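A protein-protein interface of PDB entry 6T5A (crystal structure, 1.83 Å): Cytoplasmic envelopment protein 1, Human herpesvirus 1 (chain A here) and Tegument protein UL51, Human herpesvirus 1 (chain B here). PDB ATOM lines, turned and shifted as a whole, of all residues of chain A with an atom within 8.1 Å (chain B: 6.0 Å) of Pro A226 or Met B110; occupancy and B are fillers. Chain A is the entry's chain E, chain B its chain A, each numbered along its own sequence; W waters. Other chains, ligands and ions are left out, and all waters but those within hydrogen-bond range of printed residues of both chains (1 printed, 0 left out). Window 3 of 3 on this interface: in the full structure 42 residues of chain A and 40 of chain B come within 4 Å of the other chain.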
ATOM      1  N   LEU A 220      17.334  30.789  -9.066  1.00  0.00           N
ATOM      2  CA  LEU A 220      16.457  29.652  -9.361  1.00  0.00           C
ATOM      3  C   LEU A 220      16.180  28.726  -8.173  1.00  0.00           C
ATOM      4  O   LEU A 220      15.095  28.151  -8.112  1.00  0.00           O
ATOM      5  CB  LEU A 220      16.998  28.862 -10.566  1.00  0.00           C
ATOM      6  CG  LEU A 220      17.180  29.660 -11.888  1.00  0.00           C
ATOM      7  CD1 LEU A 220      17.832  28.798 -12.966  1.00  0.00           C
ATOM      8  CD2 LEU A 220      15.859  30.302 -12.358  1.00  0.00           C
ATOM      9  N   LEU A 221      17.119  28.606  -7.218  1.00  0.00           N
ATOM     10  CA  LEU A 221      16.936  27.720  -6.056  1.00  0.00           C
ATOM     11  C   LEU A 221      16.671  28.465  -4.740  1.00  0.00           C
ATOM     12  O   LEU A 221      16.745  27.849  -3.672  1.00  0.00           O
ATOM     13  CB  LEU A 221      18.174  26.795  -5.905  1.00  0.00           C
ATOM     14  CG  LEU A 221      18.658  26.025  -7.154  1.00  0.00           C
ATOM     15  CD1 LEU A 221      19.897  25.203  -6.842  1.00  0.00           C
ATOM     16  CD2 LEU A 221      17.546  25.141  -7.738  1.00  0.00           C
ATOM     17  N   ALA A 222      16.351  29.776  -4.813  1.00  0.00           N
ATOM     18  CA  ALA A 222      16.153  30.656  -3.651  1.00  0.00           C
ATOM     19  C   ALA A 222      15.197  30.134  -2.580  1.00  0.00           C
ATOM     20  O   ALA A 222      15.537  30.182  -1.395  1.00  0.00           O
ATOM     21  CB  ALA A 222      15.714  32.038  -4.100  1.00  0.00           C
ATOM     22  N   ASN A 223      13.999  29.666  -2.984  1.00  0.00           N
ATOM     23  CA  ASN A 223      12.988  29.195  -2.045  1.00  0.00           C
ATOM     24  C   ASN A 223      12.078  28.167  -2.695  1.00  0.00           C
ATOM     25  O   ASN A 223      11.458  28.462  -3.723  1.00  0.00           O
ATOM     26  CB  ASN A 223      12.164  30.388  -1.534  1.00  0.00           C
ATOM     27  CG  ASN A 223      11.063  30.029  -0.582  1.00  0.00           C
ATOM     28  OD1 ASN A 223      11.300  29.458   0.486  1.00  0.00           O
ATOM     29  ND2 ASN A 223       9.835  30.368  -0.951  1.00  0.00           N
ATOM     30  N   ASN A 224      11.965  26.975  -2.065  1.00  0.00           N
ATOM     31  CA  ASN A 224      11.135  25.845  -2.514  1.00  0.00           C
ATOM     32  C   ASN A 224      11.192  25.670  -4.060  1.00  0.00           C
ATOM     33  O   ASN A 224      10.165  25.818  -4.737  1.00  0.00           O
ATOM     34  CB  ASN A 224       9.686  25.993  -1.982  1.00  0.00           C
ATOM     35  CG  ASN A 224       8.778  24.785  -2.148  1.00  0.00           C
ATOM     36  OD1 ASN A 224       7.548  24.913  -2.190  1.00  0.00           O
ATOM     37  ND2 ASN A 224       9.344  23.585  -2.239  1.00  0.00           N
ATOM     38  N   PRO A 225      12.398  25.451  -4.649  1.00  0.00           N
ATOM     39  CA  PRO A 225      12.475  25.331  -6.113  1.00  0.00           C
ATOM     40  C   PRO A 225      11.729  24.124  -6.680  1.00  0.00           C
ATOM     41  O   PRO A 225      11.664  23.091  -6.000  1.00  0.00           O
ATOM     42  CB  PRO A 225      13.983  25.206  -6.376  1.00  0.00           C
ATOM     43  CG  PRO A 225      14.546  24.658  -5.128  1.00  0.00           C
ATOM     44  CD  PRO A 225      13.729  25.276  -4.031  1.00  0.00           C
ATOM     45  N   PRO A 226      11.162  24.205  -7.907  1.00  0.00           N
ATOM     46  CA  PRO A 226      10.520  23.007  -8.479  1.00  0.00           C
ATOM     47  C   PRO A 226      11.588  21.968  -8.858  1.00  0.00           C
ATOM     48  O   PRO A 226      12.696  22.372  -9.227  1.00  0.00           O
ATOM     49  CB  PRO A 226       9.778  23.540  -9.706  1.00  0.00           C
ATOM     50  CG  PRO A 226      10.511  24.774 -10.098  1.00  0.00           C
ATOM     51  CD  PRO A 226      11.137  25.343  -8.852  1.00  0.00           C
ATOM     52  N   PRO A 227      11.299  20.643  -8.762  1.00  0.00           N
ATOM     53  CA  PRO A 227      12.318  19.625  -9.114  1.00  0.00           C
ATOM     54  C   PRO A 227      13.070  19.863 -10.428  1.00  0.00           C
ATOM     55  O   PRO A 227      14.286  19.657 -10.475  1.00  0.00           O
ATOM     56  CB  PRO A 227      11.516  18.322  -9.156  1.00  0.00           C
ATOM     57  CG  PRO A 227      10.391  18.547  -8.202  1.00  0.00           C
ATOM     58  CD  PRO A 227      10.040  20.010  -8.307  1.00  0.00           C
ATOM     59  N   VAL A 228      12.355  20.338 -11.474  1.00  0.00           N
ATOM     60  CA  VAL A 228      12.895  20.636 -12.807  1.00  0.00           C
ATOM     61  C   VAL A 228      14.057  21.673 -12.755  1.00  0.00           C
ATOM     62  O   VAL A 228      14.998  21.562 -13.547  1.00  0.00           O
ATOM     63  CB  VAL A 228      11.748  21.021 -13.788  1.00  0.00           C
ATOM     64  CG1 VAL A 228      11.207  22.439 -13.548  1.00  0.00           C
ATOM     65  CG2 VAL A 228      12.159  20.809 -15.240  1.00  0.00           C
ATOM     66  N   LEU A 229      14.017  22.632 -11.795  1.00  0.00           N
ATOM     67  CA  LEU A 229      15.094  23.618 -11.613  1.00  0.00           C
ATOM     68  C   LEU A 229      16.236  23.051 -10.790  1.00  0.00           C
ATOM     69  O   LEU A 229      17.404  23.258 -11.136  1.00  0.00           O
ATOM     70  CB  LEU A 229      14.594  24.968 -11.037  1.00  0.00           C
ATOM     71  CG  LEU A 229      13.819  25.880 -12.014  1.00  0.00           C
ATOM     72  CD1 LEU A 229      13.306  27.140 -11.314  1.00  0.00           C
ATOM     73  CD2 LEU A 229      14.666  26.260 -13.244  1.00  0.00           C
ATOM     74  N   SER A 230      15.908  22.306  -9.717  1.00  0.00           N
ATOM     75  CA  SER A 230      16.903  21.650  -8.858  1.00  0.00           C
ATOM     76  C   SER A 230      17.728  20.627  -9.656  1.00  0.00           C
ATOM     77  O   SER A 230      18.918  20.476  -9.400  1.00  0.00           O
ATOM     78  CB  SER A 230      16.221  20.957  -7.682  1.00  0.00           C
ATOM     79  OG  SER A 230      15.457  21.884  -6.932  1.00  0.00           O
ATOM     80  N   ALA A 231      17.101  19.975 -10.658  1.00  0.00           N
ATOM     81  CA  ALA A 231      17.724  18.969 -11.534  1.00  0.00           C
ATOM     82  C   ALA A 231      18.896  19.512 -12.358  1.00  0.00           C
ATOM     83  O   ALA A 231      19.785  18.741 -12.721  1.00  0.00           O
ATOM     84  CB  ALA A 231      16.678  18.348 -12.446  1.00  0.00           C
ATOM     85  N   LEU A 232      18.916  20.840 -12.630  1.00  0.00           N
ATOM     86  CA  LEU A 232      19.994  21.492 -13.390  1.00  0.00           C
ATOM     87  C   LEU A 232      21.310  21.550 -12.613  1.00  0.00           C
ATOM     88  O   LEU A 232      22.374  21.739 -13.205  1.00  0.00           O
ATOM     89  CB  LEU A 232      19.598  22.933 -13.775  1.00  0.00           C
ATOM     90  CG  LEU A 232      18.348  23.115 -14.621  1.00  0.00           C
ATOM     91  CD1 LEU A 232      17.989  24.584 -14.748  1.00  0.00           C
ATOM     92  CD2 LEU A 232      18.502  22.452 -15.993  1.00  0.00           C
ATOM     93  N   TYR B  69      12.660  35.774 -13.335  1.00  0.00           N
ATOM     94  CA  TYR B  69      12.033  34.672 -12.603  1.00  0.00           C
ATOM     95  C   TYR B  69      11.956  35.042 -11.121  1.00  0.00           C
ATOM     96  O   TYR B  69      10.899  34.905 -10.503  1.00  0.00           O
ATOM     97  CB  TYR B  69      12.835  33.372 -12.813  1.00  0.00           C
ATOM     98  CG  TYR B  69      12.353  32.224 -11.955  1.00  0.00           C
ATOM     99  CD1 TYR B  69      11.278  31.434 -12.354  1.00  0.00           C
ATOM    100  CD2 TYR B  69      12.951  31.947 -10.729  1.00  0.00           C
ATOM    101  CE1 TYR B  69      10.814  30.391 -11.557  1.00  0.00           C
ATOM    102  CE2 TYR B  69      12.500  30.903  -9.926  1.00  0.00           C
ATOM    103  CZ  TYR B  69      11.431  30.129 -10.344  1.00  0.00           C
ATOM    104  OH  TYR B  69      10.988  29.093  -9.569  1.00  0.00           O
ATOM    105  N   LEU B 105       4.470  34.248 -16.320  1.00  0.00           N
ATOM    106  CA  LEU B 105       5.739  34.864 -16.700  1.00  0.00           C
ATOM    107  C   LEU B 105       6.918  34.063 -16.135  1.00  0.00           C
ATOM    108  O   LEU B 105       7.879  33.819 -16.871  1.00  0.00           O
ATOM    109  CB  LEU B 105       5.803  36.366 -16.338  1.00  0.00           C
ATOM    110  CG  LEU B 105       7.088  37.156 -16.755  1.00  0.00           C
ATOM    111  CD1 LEU B 105       7.350  37.108 -18.275  1.00  0.00           C
ATOM    112  CD2 LEU B 105       7.023  38.603 -16.288  1.00  0.00           C
ATOM    113  N   ALA B 106       6.815  33.589 -14.866  1.00  0.00           N
ATOM    114  CA  ALA B 106       7.846  32.753 -14.238  1.00  0.00           C
ATOM    115  C   ALA B 106       8.006  31.444 -15.032  1.00  0.00           C
ATOM    116  O   ALA B 106       9.136  31.039 -15.305  1.00  0.00           O
ATOM    117  CB  ALA B 106       7.490  32.457 -12.790  1.00  0.00           C
ATOM    118  N   ASP B 107       6.875  30.822 -15.454  1.00  0.00           N
ATOM    119  CA  ASP B 107       6.893  29.598 -16.267  1.00  0.00           C
ATOM    120  C   ASP B 107       7.623  29.819 -17.594  1.00  0.00           C
ATOM    121  O   ASP B 107       8.417  28.973 -17.994  1.00  0.00           O
ATOM    122  CB  ASP B 107       5.457  29.082 -16.524  1.00  0.00           C
ATOM    123  CG  ASP B 107       4.779  28.411 -15.336  1.00  0.00           C
ATOM    124  OD1 ASP B 107       5.464  28.162 -14.317  1.00  0.00           O
ATOM    125  OD2 ASP B 107       3.565  28.136 -15.425  1.00  0.00           O
ATOM    126  N   THR B 108       7.384  30.976 -18.249  1.00  0.00           N
ATOM    127  CA  THR B 108       8.040  31.354 -19.511  1.00  0.00           C
ATOM    128  C   THR B 108       9.562  31.487 -19.319  1.00  0.00           C
ATOM    129  O   THR B 108      10.326  30.965 -20.134  1.00  0.00           O
ATOM    130  CB  THR B 108       7.366  32.606 -20.096  1.00  0.00           C
ATOM    131  OG1 THR B 108       5.995  32.293 -20.318  1.00  0.00           O
ATOM    132  CG2 THR B 108       7.980  33.052 -21.409  1.00  0.00           C
ATOM    133  N   CYS B 109       9.993  32.144 -18.217  1.00  0.00           N
ATOM    134  CA  CYS B 109      11.410  32.313 -17.870  1.00  0.00           C
ATOM    135  C   CYS B 109      12.051  30.974 -17.652  1.00  0.00           C
ATOM    136  O   CYS B 109      13.139  30.730 -18.165  1.00  0.00           O
ATOM    137  CB  CYS B 109      11.569  33.199 -16.640  1.00  0.00           C
ATOM    138  SG  CYS B 109      11.171  34.931 -16.936  1.00  0.00           S
ATOM    139  N   MET B 110      11.376  30.112 -16.879  1.00  0.00           N
ATOM    140  CA  MET B 110      11.836  28.774 -16.554  1.00  0.00           C
ATOM    141  C   MET B 110      11.995  27.942 -17.824  1.00  0.00           C
ATOM    142  O   MET B 110      13.046  27.330 -17.981  1.00  0.00           O
ATOM    143  CB  MET B 110      10.874  28.110 -15.570  1.00  0.00           C
ATOM    144  CG  MET B 110      11.457  26.922 -14.862  1.00  0.00           C
ATOM    145  SD  MET B 110      10.251  26.019 -13.857  1.00  0.00           S
ATOM    146  CE  MET B 110       9.610  27.323 -12.834  1.00  0.00           C
ATOM    147  N   ALA B 111      10.992  27.975 -18.747  1.00  0.00           N
ATOM    148  CA  ALA B 111      11.025  27.255 -20.027  1.00  0.00           C
ATOM    149  C   ALA B 111      12.233  27.654 -20.890  1.00  0.00           C
ATOM    150  O   ALA B 111      12.876  26.775 -21.461  1.00  0.00           O
ATOM    151  CB  ALA B 111       9.730  27.476 -20.800  1.00  0.00           C
ATOM    152  N   THR B 112      12.549  28.969 -20.969  1.00  0.00           N
ATOM    153  CA  THR B 112      13.686  29.492 -21.742  1.00  0.00           C
ATOM    154  C   THR B 112      15.031  29.051 -21.141  1.00  0.00           C
ATOM    155  O   THR B 112      15.956  28.719 -21.890  1.00  0.00           O
ATOM    156  CB  THR B 112      13.564  31.012 -21.917  1.00  0.00           C
ATOM    157  OG1 THR B 112      12.254  31.298 -22.393  1.00  0.00           O
ATOM    158  CG2 THR B 112      14.591  31.582 -22.896  1.00  0.00           C
ATOM    159  N   ILE B 113      15.136  29.058 -19.792  1.00  0.00           N
ATOM    160  CA  ILE B 113      16.343  28.635 -19.075  1.00  0.00           C
ATOM    161  C   ILE B 113      16.560  27.135 -19.310  1.00  0.00           C
ATOM    162  O   ILE B 113      17.680  26.733 -19.629  1.00  0.00           O
ATOM    163  CB  ILE B 113      16.284  29.002 -17.561  1.00  0.00           C
ATOM    164  CG1 ILE B 113      16.281  30.536 -17.366  1.00  0.00           C
ATOM    165  CG2 ILE B 113      17.427  28.327 -16.766  1.00  0.00           C
ATOM    166  CD1 ILE B 113      15.825  31.029 -15.980  1.00  0.00           C
ATOM    167  N   LEU B 114      15.485  26.326 -19.201  1.00  0.00           N
ATOM    168  CA  LEU B 114      15.557  24.877 -19.417  1.00  0.00           C
ATOM    169  C   LEU B 114      15.985  24.510 -20.834  1.00  0.00           C
ATOM    170  O   LEU B 114      16.725  23.543 -20.997  1.00  0.00           O
ATOM    171  CB  LEU B 114      14.242  24.178 -19.063  1.00  0.00           C
ATOM    172  CG  LEU B 114      13.866  24.144 -17.577  1.00  0.00           C
ATOM    173  CD1 LEU B 114      12.376  23.852 -17.404  1.00  0.00           C
ATOM    174  CD2 LEU B 114      14.709  23.144 -16.814  1.00  0.00           C
ATOM    175  N   GLN B 115      15.547  25.285 -21.845  1.00  0.00           N
ATOM    176  CA  GLN B 115      15.896  25.074 -23.251  1.00  0.00           C
ATOM    177  C   GLN B 115      17.397  25.306 -23.475  1.00  0.00           C
ATOM    178  O   GLN B 115      18.037  24.522 -24.181  1.00  0.00           O
ATOM    179  CB  GLN B 115      15.035  25.969 -24.159  1.00  0.00           C
ATOM    180  CG  GLN B 115      15.109  25.612 -25.643  1.00  0.00           C
ATOM    181  CD  GLN B 115      14.155  26.412 -26.504  1.00  0.00           C
ATOM    182  OE1 GLN B 115      13.566  27.422 -26.085  1.00  0.00           O
ATOM    183  NE2 GLN B 115      13.985  25.972 -27.741  1.00  0.00           N
HETATM  184  O   HOH W   1      12.063  28.923  -7.077  1.00  0.00           O
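Among the printed residues, pairs that only touch across the chains: Leu A229 with Tyr B69 (3.5 Å), Val A228 with Leu B114 (3.6 Å), Leu A229 with Met B110 (3.7 Å), Leu A220 with Ile B113 (3.7 Å), Leu A220 with Tyr B69 (3.7 Å), Val A228 with Met B110 (3.7 Å), Pro A226 with Tyr B69 (3.8 Å), Pro A226 with Met B110 (3.8 Å) and Leu A232 with Leu B114 (3.9 Å).
Water W1 lies within hydrogen-bond range of the side-chain hydroxyl (OH) of Tyr B69, the backbone carbonyl oxygen (O) of Leu A220 and the backbone carbonyl oxygen (O) of Asn A223.
Of the 12 printed residues of chain B, 4 touch a printed residue of chain A.
Hydrophobic or aromatic side chains of chain B that line the printed part of chain A: Tyr B69, Met B110, Ile B113 and Leu B114.
Hydrophobic or aromatic side chains of chain A that line the printed part of chain B: Leu A220, Pro A226, Val A228, Leu A229 and Leu A232.
Along chain A the printed residues that touch a printed residue of chain B span positions 220 to 232.
Among the printed residues, no Asp or Glu carboxylate lies within 4 Å of a Lys or Arg side-chain nitrogen of the other chain.
Pro A226 touches just these residues of chain B: Tyr B69 and Met B110.
Met B110 touches just these residues of chain A: Pro A226, Val A228 and Leu A229.
No residue of chain A comes within 4 Å of Ala B111.
Of the printed residues of chain B, Leu A229 touches Tyr B69 and Met B110.
Of the printed residues of chain A, Tyr B69 touches Leu A220, Pro A226 and Leu A229.
Of the printed residues of chain B, Val A228 touches Met B110 (3.7 Å) and Leu B114 (3.6 Å).
Of the printed residues of chain A, Leu B114 touches Val A228 (3.6 Å) and Leu A232 (3.9 Å).
Printed residues of chain A within 4 Å of Ile B113: Leu A220.
Asp B107 touches none of the printed residues of chain A.
Asn A224 touches none of the printed residues of chain B.
The nearest printed residue of chain B that does not touch Pro A226 is Asp B107 (7.4 Å).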
